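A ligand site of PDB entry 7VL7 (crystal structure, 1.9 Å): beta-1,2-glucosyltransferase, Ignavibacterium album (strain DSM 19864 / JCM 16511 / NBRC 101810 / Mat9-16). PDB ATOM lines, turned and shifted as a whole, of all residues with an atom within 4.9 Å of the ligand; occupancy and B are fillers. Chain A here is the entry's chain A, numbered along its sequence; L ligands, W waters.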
ATOM      1  N   LEU A  95     -16.571   6.799   8.332  1.00  0.00           N
ATOM      2  CA  LEU A  95     -16.394   8.263   8.199  1.00  0.00           C
ATOM      3  C   LEU A  95     -16.392   8.862   9.611  1.00  0.00           C
ATOM      4  O   LEU A  95     -15.352   8.741  10.293  1.00  0.00           O
ATOM      5  CB  LEU A  95     -17.482   8.807   7.262  1.00  0.00           C
ATOM      6  CG  LEU A  95     -17.602   8.044   5.932  1.00  0.00           C
ATOM      7  CD1 LEU A  95     -18.579   8.747   4.987  1.00  0.00           C
ATOM      8  CD2 LEU A  95     -16.247   7.875   5.233  1.00  0.00           C
ATOM      9  N   GLU A  97     -16.056  11.575  11.242  1.00  0.00           N
ATOM     10  CA  GLU A  97     -14.953  12.494  11.659  1.00  0.00           C
ATOM     11  C   GLU A  97     -13.846  11.714  12.392  1.00  0.00           C
ATOM     12  O   GLU A  97     -13.227  12.279  13.316  1.00  0.00           O
ATOM     13  CB  GLU A  97     -15.524  13.625  12.534  1.00  0.00           C
ATOM     14  CG  GLU A  97     -16.270  14.710  11.748  1.00  0.00           C
ATOM     15  CD  GLU A  97     -17.627  14.351  11.143  1.00  0.00           C
ATOM     16  OE1 GLU A  97     -18.006  14.958  10.122  1.00  0.00           O
ATOM     17  OE2 GLU A  97     -18.304  13.439  11.686  1.00  0.00           O
ATOM     18  N   GLN A 101     -11.109   8.018   8.196  1.00  0.00           N
ATOM     19  CA  GLN A 101     -12.539   7.632   8.030  1.00  0.00           C
ATOM     20  C   GLN A 101     -12.825   6.232   8.606  1.00  0.00           C
ATOM     21  O   GLN A 101     -13.815   5.619   8.145  1.00  0.00           O
ATOM     22  CB  GLN A 101     -12.941   7.649   6.552  1.00  0.00           C
ATOM     23  CG  GLN A 101     -12.459   8.874   5.772  1.00  0.00           C
ATOM     24  CD  GLN A 101     -13.011  10.157   6.334  1.00  0.00           C
ATOM     25  OE1 GLN A 101     -14.110  10.202   6.894  1.00  0.00           O
ATOM     26  NE2 GLN A 101     -12.242  11.217   6.186  1.00  0.00           N
ATOM     27  N   GLU A 171     -22.529   5.288   3.780  1.00  0.00           N
ATOM     28  CA  GLU A 171     -22.770   6.261   2.680  1.00  0.00           C
ATOM     29  C   GLU A 171     -21.893   5.894   1.480  1.00  0.00           C
ATOM     30  O   GLU A 171     -20.996   6.667   1.069  1.00  0.00           O
ATOM     31  CB  GLU A 171     -22.502   7.678   3.171  1.00  0.00           C
ATOM     32  CG  GLU A 171     -23.436   8.127   4.290  1.00  0.00           C
ATOM     33  CD  GLU A 171     -23.152   9.528   4.798  1.00  0.00           C
ATOM     34  OE1 GLU A 171     -22.033   9.999   4.574  1.00  0.00           O
ATOM     35  OE2 GLU A 171     -24.114  10.207   5.342  1.00  0.00           O
ATOM     36  N   VAL A 174     -20.071   8.483  -0.953  1.00  0.00           N
ATOM     37  CA  VAL A 174     -20.034   9.885  -0.437  1.00  0.00           C
ATOM     38  C   VAL A 174     -18.622  10.460  -0.547  1.00  0.00           C
ATOM     39  O   VAL A 174     -18.476  11.634  -0.866  1.00  0.00           O
ATOM     40  CB  VAL A 174     -20.578  10.024   1.002  1.00  0.00           C
ATOM     41  CG1 VAL A 174     -19.593   9.575   2.059  1.00  0.00           C
ATOM     42  CG2 VAL A 174     -21.008  11.462   1.251  1.00  0.00           C
ATOM     43  N   PHE A 175     -17.615   9.662  -0.205  1.00  0.00           N
ATOM     44  CA  PHE A 175     -16.205  10.100  -0.222  1.00  0.00           C
ATOM     45  C   PHE A 175     -15.826  10.416  -1.676  1.00  0.00           C
ATOM     46  O   PHE A 175     -15.319  11.518  -1.942  1.00  0.00           O
ATOM     47  CB  PHE A 175     -15.347   9.079   0.556  1.00  0.00           C
ATOM     48  CG  PHE A 175     -13.969   9.561   0.975  1.00  0.00           C
ATOM     49  CD1 PHE A 175     -13.412  10.729   0.463  1.00  0.00           C
ATOM     50  CD2 PHE A 175     -13.181   8.756   1.807  1.00  0.00           C
ATOM     51  CE1 PHE A 175     -12.127  11.131   0.819  1.00  0.00           C
ATOM     52  CE2 PHE A 175     -11.909   9.170   2.163  1.00  0.00           C
ATOM     53  CZ  PHE A 175     -11.379  10.343   1.658  1.00  0.00           C
ATOM     54  N   TRP A 177     -17.796  11.299  -4.072  1.00  0.00           N
ATOM     55  CA  TRP A 177     -18.563  12.519  -4.402  1.00  0.00           C
ATOM     56  C   TRP A 177     -17.846  13.780  -3.892  1.00  0.00           C
ATOM     57  O   TRP A 177     -17.633  14.687  -4.696  1.00  0.00           O
ATOM     58  CB  TRP A 177     -19.971  12.358  -3.800  1.00  0.00           C
ATOM     59  CG  TRP A 177     -20.864  13.557  -3.863  1.00  0.00           C
ATOM     60  CD1 TRP A 177     -21.346  14.185  -4.970  1.00  0.00           C
ATOM     61  CD2 TRP A 177     -21.507  14.165  -2.742  1.00  0.00           C
ATOM     62  NE1 TRP A 177     -22.226  15.168  -4.599  1.00  0.00           N
ATOM     63  CE2 TRP A 177     -22.346  15.189  -3.248  1.00  0.00           C
ATOM     64  CE3 TRP A 177     -21.443  13.979  -1.366  1.00  0.00           C
ATOM     65  CZ2 TRP A 177     -23.128  15.990  -2.418  1.00  0.00           C
ATOM     66  CZ3 TRP A 177     -22.230  14.747  -0.538  1.00  0.00           C
ATOM     67  CH2 TRP A 177     -23.028  15.773  -1.057  1.00  0.00           C
ATOM     68  N   LEU A 178     -17.510  13.840  -2.600  1.00  0.00           N
ATOM     69  CA  LEU A 178     -16.883  15.039  -1.958  1.00  0.00           C
ATOM     70  C   LEU A 178     -15.486  15.256  -2.553  1.00  0.00           C
ATOM     71  O   LEU A 178     -15.069  16.435  -2.657  1.00  0.00           O
ATOM     72  CB  LEU A 178     -16.812  14.827  -0.443  1.00  0.00           C
ATOM     73  CG  LEU A 178     -18.162  14.786   0.296  1.00  0.00           C
ATOM     74  CD1 LEU A 178     -17.970  14.528   1.769  1.00  0.00           C
ATOM     75  CD2 LEU A 178     -18.922  16.079   0.139  1.00  0.00           C
ATOM     76  N   PRO A 272     -26.426   9.709   1.984  1.00  0.00           N
ATOM     77  CA  PRO A 272     -25.867  11.060   2.121  1.00  0.00           C
ATOM     78  C   PRO A 272     -26.513  12.044   1.140  1.00  0.00           C
ATOM     79  O   PRO A 272     -27.273  11.617   0.272  1.00  0.00           O
ATOM     80  CB  PRO A 272     -24.399  10.810   1.750  1.00  0.00           C
ATOM     81  CG  PRO A 272     -24.510   9.777   0.649  1.00  0.00           C
ATOM     82  CD  PRO A 272     -25.679   8.892   1.013  1.00  0.00           C
ATOM     83  N   GLY A 273     -26.213  13.341   1.277  1.00  0.00           N
ATOM     84  CA  GLY A 273     -26.698  14.314   0.301  1.00  0.00           C
ATOM     85  C   GLY A 273     -26.839  15.709   0.847  1.00  0.00           C
ATOM     86  O   GLY A 273     -26.805  16.625   0.029  1.00  0.00           O
ATOM     87  N   TRP A 274     -27.065  15.879   2.145  1.00  0.00           N
ATOM     88  CA  TRP A 274     -27.206  17.257   2.674  1.00  0.00           C
ATOM     89  C   TRP A 274     -25.840  17.922   2.685  1.00  0.00           C
ATOM     90  O   TRP A 274     -24.828  17.260   3.049  1.00  0.00           O
ATOM     91  CB  TRP A 274     -27.802  17.268   4.070  1.00  0.00           C
ATOM     92  CG  TRP A 274     -29.230  16.881   4.167  1.00  0.00           C
ATOM     93  CD1 TRP A 274     -29.736  15.616   4.102  1.00  0.00           C
ATOM     94  CD2 TRP A 274     -30.344  17.756   4.425  1.00  0.00           C
ATOM     95  NE1 TRP A 274     -31.081  15.646   4.304  1.00  0.00           N
ATOM     96  CE2 TRP A 274     -31.485  16.938   4.542  1.00  0.00           C
ATOM     97  CE3 TRP A 274     -30.469  19.126   4.643  1.00  0.00           C
ATOM     98  CZ2 TRP A 274     -32.740  17.449   4.825  1.00  0.00           C
ATOM     99  CZ3 TRP A 274     -31.719  19.643   4.914  1.00  0.00           C
ATOM    100  CH2 TRP A 274     -32.840  18.812   4.999  1.00  0.00           C
ATOM    101  N   ILE A 275     -25.778  19.182   2.290  1.00  0.00           N
ATOM    102  CA  ILE A 275     -24.524  19.952   2.475  1.00  0.00           C
ATOM    103  C   ILE A 275     -24.951  21.405   2.595  1.00  0.00           C
ATOM    104  O   ILE A 275     -25.887  21.789   1.894  1.00  0.00           O
ATOM    105  CB  ILE A 275     -23.542  19.667   1.319  1.00  0.00           C
ATOM    106  CG1 ILE A 275     -22.173  20.307   1.554  1.00  0.00           C
ATOM    107  CG2 ILE A 275     -24.139  20.057  -0.023  1.00  0.00           C
ATOM    108  CD1 ILE A 275     -21.129  19.888   0.541  1.00  0.00           C
ATOM    109  N   ASP A 304     -29.780  10.337   6.004  1.00  0.00           N
ATOM    110  CA  ASP A 304     -28.894  11.138   6.871  1.00  0.00           C
ATOM    111  C   ASP A 304     -29.277  12.609   6.725  1.00  0.00           C
ATOM    112  O   ASP A 304     -28.734  13.260   5.845  1.00  0.00           O
ATOM    113  CB  ASP A 304     -27.422  10.841   6.547  1.00  0.00           C
ATOM    114  CG  ASP A 304     -27.050   9.368   6.774  1.00  0.00           C
ATOM    115  OD1 ASP A 304     -27.853   8.621   7.420  1.00  0.00           O
ATOM    116  OD2 ASP A 304     -25.898   8.981   6.339  1.00  0.00           O
ATOM    117  N   ILE A 306     -29.212  16.445   7.662  1.00  0.00           N
ATOM    118  CA  ILE A 306     -28.357  17.491   8.284  1.00  0.00           C
ATOM    119  C   ILE A 306     -28.871  18.870   7.858  1.00  0.00           C
ATOM    120  O   ILE A 306     -28.248  19.569   7.071  1.00  0.00           O
ATOM    121  CB  ILE A 306     -26.875  17.334   7.909  1.00  0.00           C
ATOM    122  CG1 ILE A 306     -26.416  15.875   7.898  1.00  0.00           C
ATOM    123  CG2 ILE A 306     -26.009  18.182   8.843  1.00  0.00           C
ATOM    124  CD1 ILE A 306     -25.011  15.722   7.372  1.00  0.00           C
ATOM    125  N   GLU A 338     -29.442   8.784  10.370  1.00  0.00           N
ATOM    126  CA  GLU A 338     -28.732   9.878  11.094  1.00  0.00           C
ATOM    127  C   GLU A 338     -29.662  11.079  11.057  1.00  0.00           C
ATOM    128  O   GLU A 338     -30.013  11.542   9.938  1.00  0.00           O
ATOM    129  CB  GLU A 338     -27.373  10.209  10.479  1.00  0.00           C
ATOM    130  CG  GLU A 338     -26.446   9.008  10.339  1.00  0.00           C
ATOM    131  CD  GLU A 338     -25.151   9.273   9.586  1.00  0.00           C
ATOM    132  OE1 GLU A 338     -24.819  10.456   9.304  1.00  0.00           O
ATOM    133  OE2 GLU A 338     -24.530   8.277   9.185  1.00  0.00           O
ATOM    134  N   ARG A 344     -21.794  18.723  13.813  1.00  0.00           N
ATOM    135  CA  ARG A 344     -20.498  18.077  13.548  1.00  0.00           C
ATOM    136  C   ARG A 344     -19.342  19.078  13.528  1.00  0.00           C
ATOM    137  O   ARG A 344     -18.157  18.643  13.556  1.00  0.00           O
ATOM    138  CB  ARG A 344     -20.621  17.378  12.190  1.00  0.00           C
ATOM    139  CG  ARG A 344     -20.851  18.347  11.049  1.00  0.00           C
ATOM    140  CD  ARG A 344     -21.127  17.498   9.832  1.00  0.00           C
ATOM    141  NE  ARG A 344     -21.544  18.284   8.676  1.00  0.00           N
ATOM    142  CZ  ARG A 344     -21.520  17.838   7.428  1.00  0.00           C
ATOM    143  NH1 ARG A 344     -21.882  18.637   6.438  1.00  0.00           N
ATOM    144  NH2 ARG A 344     -21.097  16.609   7.163  1.00  0.00           N
ATOM    145  N   PHE A 386     -10.516  13.336  13.313  1.00  0.00           N
ATOM    146  CA  PHE A 386     -10.033  13.761  11.978  1.00  0.00           C
ATOM    147  C   PHE A 386      -9.710  15.262  12.007  1.00  0.00           C
ATOM    148  O   PHE A 386      -8.742  15.650  11.375  1.00  0.00           O
ATOM    149  CB  PHE A 386     -11.072  13.424  10.887  1.00  0.00           C
ATOM    150  CG  PHE A 386     -10.522  13.456   9.482  1.00  0.00           C
ATOM    151  CD1 PHE A 386     -10.508  14.637   8.741  1.00  0.00           C
ATOM    152  CD2 PHE A 386     -10.007  12.295   8.896  1.00  0.00           C
ATOM    153  CE1 PHE A 386      -9.983  14.663   7.461  1.00  0.00           C
ATOM    154  CE2 PHE A 386      -9.489  12.330   7.607  1.00  0.00           C
ATOM    155  CZ  PHE A 386      -9.477  13.509   6.891  1.00  0.00           C
ATOM    156  N   TYR A 387     -10.525  16.066  12.692  1.00  0.00           N
ATOM    157  CA  TYR A 387     -10.611  17.547  12.550  1.00  0.00           C
ATOM    158  C   TYR A 387     -10.393  18.290  13.875  1.00  0.00           C
ATOM    159  O   TYR A 387     -10.548  19.517  13.871  1.00  0.00           O
ATOM    160  CB  TYR A 387     -12.002  18.009  12.084  1.00  0.00           C
ATOM    161  CG  TYR A 387     -12.422  17.679  10.676  1.00  0.00           C
ATOM    162  CD1 TYR A 387     -11.607  17.953   9.584  1.00  0.00           C
ATOM    163  CD2 TYR A 387     -13.694  17.173  10.421  1.00  0.00           C
ATOM    164  CE1 TYR A 387     -12.015  17.683   8.283  1.00  0.00           C
ATOM    165  CE2 TYR A 387     -14.125  16.894   9.122  1.00  0.00           C
ATOM    166  CZ  TYR A 387     -13.276  17.154   8.056  1.00  0.00           C
ATOM    167  OH  TYR A 387     -13.683  16.860   6.779  1.00  0.00           O
HETATM  168  O1  LIG L   1     -19.618  13.882   6.088  1.00  0.00           O
HETATM  169  O2  LIG L   1     -20.769  15.180   4.540  1.00  0.00           O
HETATM  170  O3  LIG L   1     -14.298  14.305   4.585  1.00  0.00           O
HETATM  171  O4  LIG L   1     -21.732  11.927   6.096  1.00  0.00           O
HETATM  172  O5  LIG L   1     -24.214  12.889   5.096  1.00  0.00           O
HETATM  173  O6  LIG L   1     -23.978  14.761   2.787  1.00  0.00           O
HETATM  174  O7  LIG L   1     -18.248  16.143   6.465  1.00  0.00           O
HETATM  175  O8  LIG L   1     -12.442  13.499   3.737  1.00  0.00           O
HETATM  176  O9  LIG L   1     -22.342  17.534   3.865  1.00  0.00           O
HETATM  177  C1  LIG L   1     -20.587  13.840   5.031  1.00  0.00           C
HETATM  178  C2  LIG L   1     -21.895  13.262   5.594  1.00  0.00           C
HETATM  179  C3  LIG L   1     -18.287  13.938   5.706  1.00  0.00           C
HETATM  180  C4  LIG L   1     -22.973  13.322   4.502  1.00  0.00           C
HETATM  181  C5  LIG L   1     -23.090  14.741   3.919  1.00  0.00           C
HETATM  182  C6  LIG L   1     -21.716  15.213   3.429  1.00  0.00           C
HETATM  183  C7  LIG L   1     -16.298  12.955   4.725  1.00  0.00           C
HETATM  184  C8  LIG L   1     -15.628  14.156   4.944  1.00  0.00           C
HETATM  185  C9  LIG L   1     -17.579  15.128   5.902  1.00  0.00           C
HETATM  186  C10 LIG L   1     -17.660  12.867   5.127  1.00  0.00           C
HETATM  187  C11 LIG L   1     -16.249  15.250   5.529  1.00  0.00           C
HETATM  188  C12 LIG L   1     -15.558  11.881   4.132  1.00  0.00           C
HETATM  189  C13 LIG L   1     -13.593  13.270   4.003  1.00  0.00           C
HETATM  190  C14 LIG L   1     -21.731  16.626   2.911  1.00  0.00           C
HETATM  191  C15 LIG L   1     -14.269  12.036   3.781  1.00  0.00           C
HETATM  192  O   HOH W   1     -19.374  11.806   7.882  1.00  0.00           O
HETATM  193  O   HOH W   2     -26.540  14.153   4.405  1.00  0.00           O
HETATM  194  O   HOH W   3     -20.037  14.420   8.910  1.00  0.00           O
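O of Gln 101 lies within hydrogen-bond range of N of Leu 95 (3.0 Å).
N of Phe 386 is in hydrogen-bond range of O of Glu 97 (2.9 Å).
The backbone NH (N) of Gly 273 sits at hydrogen-bond distance from an oxygen (O6) of the ligand, at 3.0 Å.
OE1 of Glu 171 is in hydrogen-bond range of O4 of the ligand (2.5 Å).
N of Trp 274 lies within hydrogen-bond range of O6 of the ligand, 3.3 Å away.
The guanidinium group (NH1) of Arg 344 is in hydrogen-bond range of an oxygen (O9) of the ligand (2.8 Å).
The side-chain amide nitrogen (NE2) of Gln 101 sits close to an oxygen (O8) of the ligand (3.4 Å).
An oxygen (O9) of the ligand sits at hydrogen-bond distance from the backbone carbonyl oxygen of Trp 274 (2.6 Å).
OH of Tyr 387 sits close to O3 of the ligand (3.4 Å).
Merely in contact with the ligand: Glu 97 (3.9 Å), Phe 175 (3.7 Å), Trp 177 (3.8 Å), Leu 178 (3.7 Å), Pro 272 (3.9 Å), Ile 275 (3.5 Å) and Ile 306 (3.7 Å).
Hydrophobic or aromatic side chains within 4 Å of the ligand: Phe 175, Trp 177, Leu 178, Pro 272, Ile 275 and Ile 306.
Of the 18 residues printed, 13 come within 4 Å of the ligand.
Along chain A the residues within 4 Å of the ligand span positions 97 to 387.
Water W2 lies within hydrogen-bond range of an oxygen (O5) of the ligand (2.7 Å), the backbone carbonyl oxygen of Asp 304 (2.8 Å), the backbone NH of Trp 274 (2.9 Å) and the backbone NH of Gly 273 (3.2 Å).
Water W3 lies within hydrogen-bond range of the side-chain carboxylate of Glu 97, an oxygen (O1) of the ligand and the guanidinium group of Arg 344.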
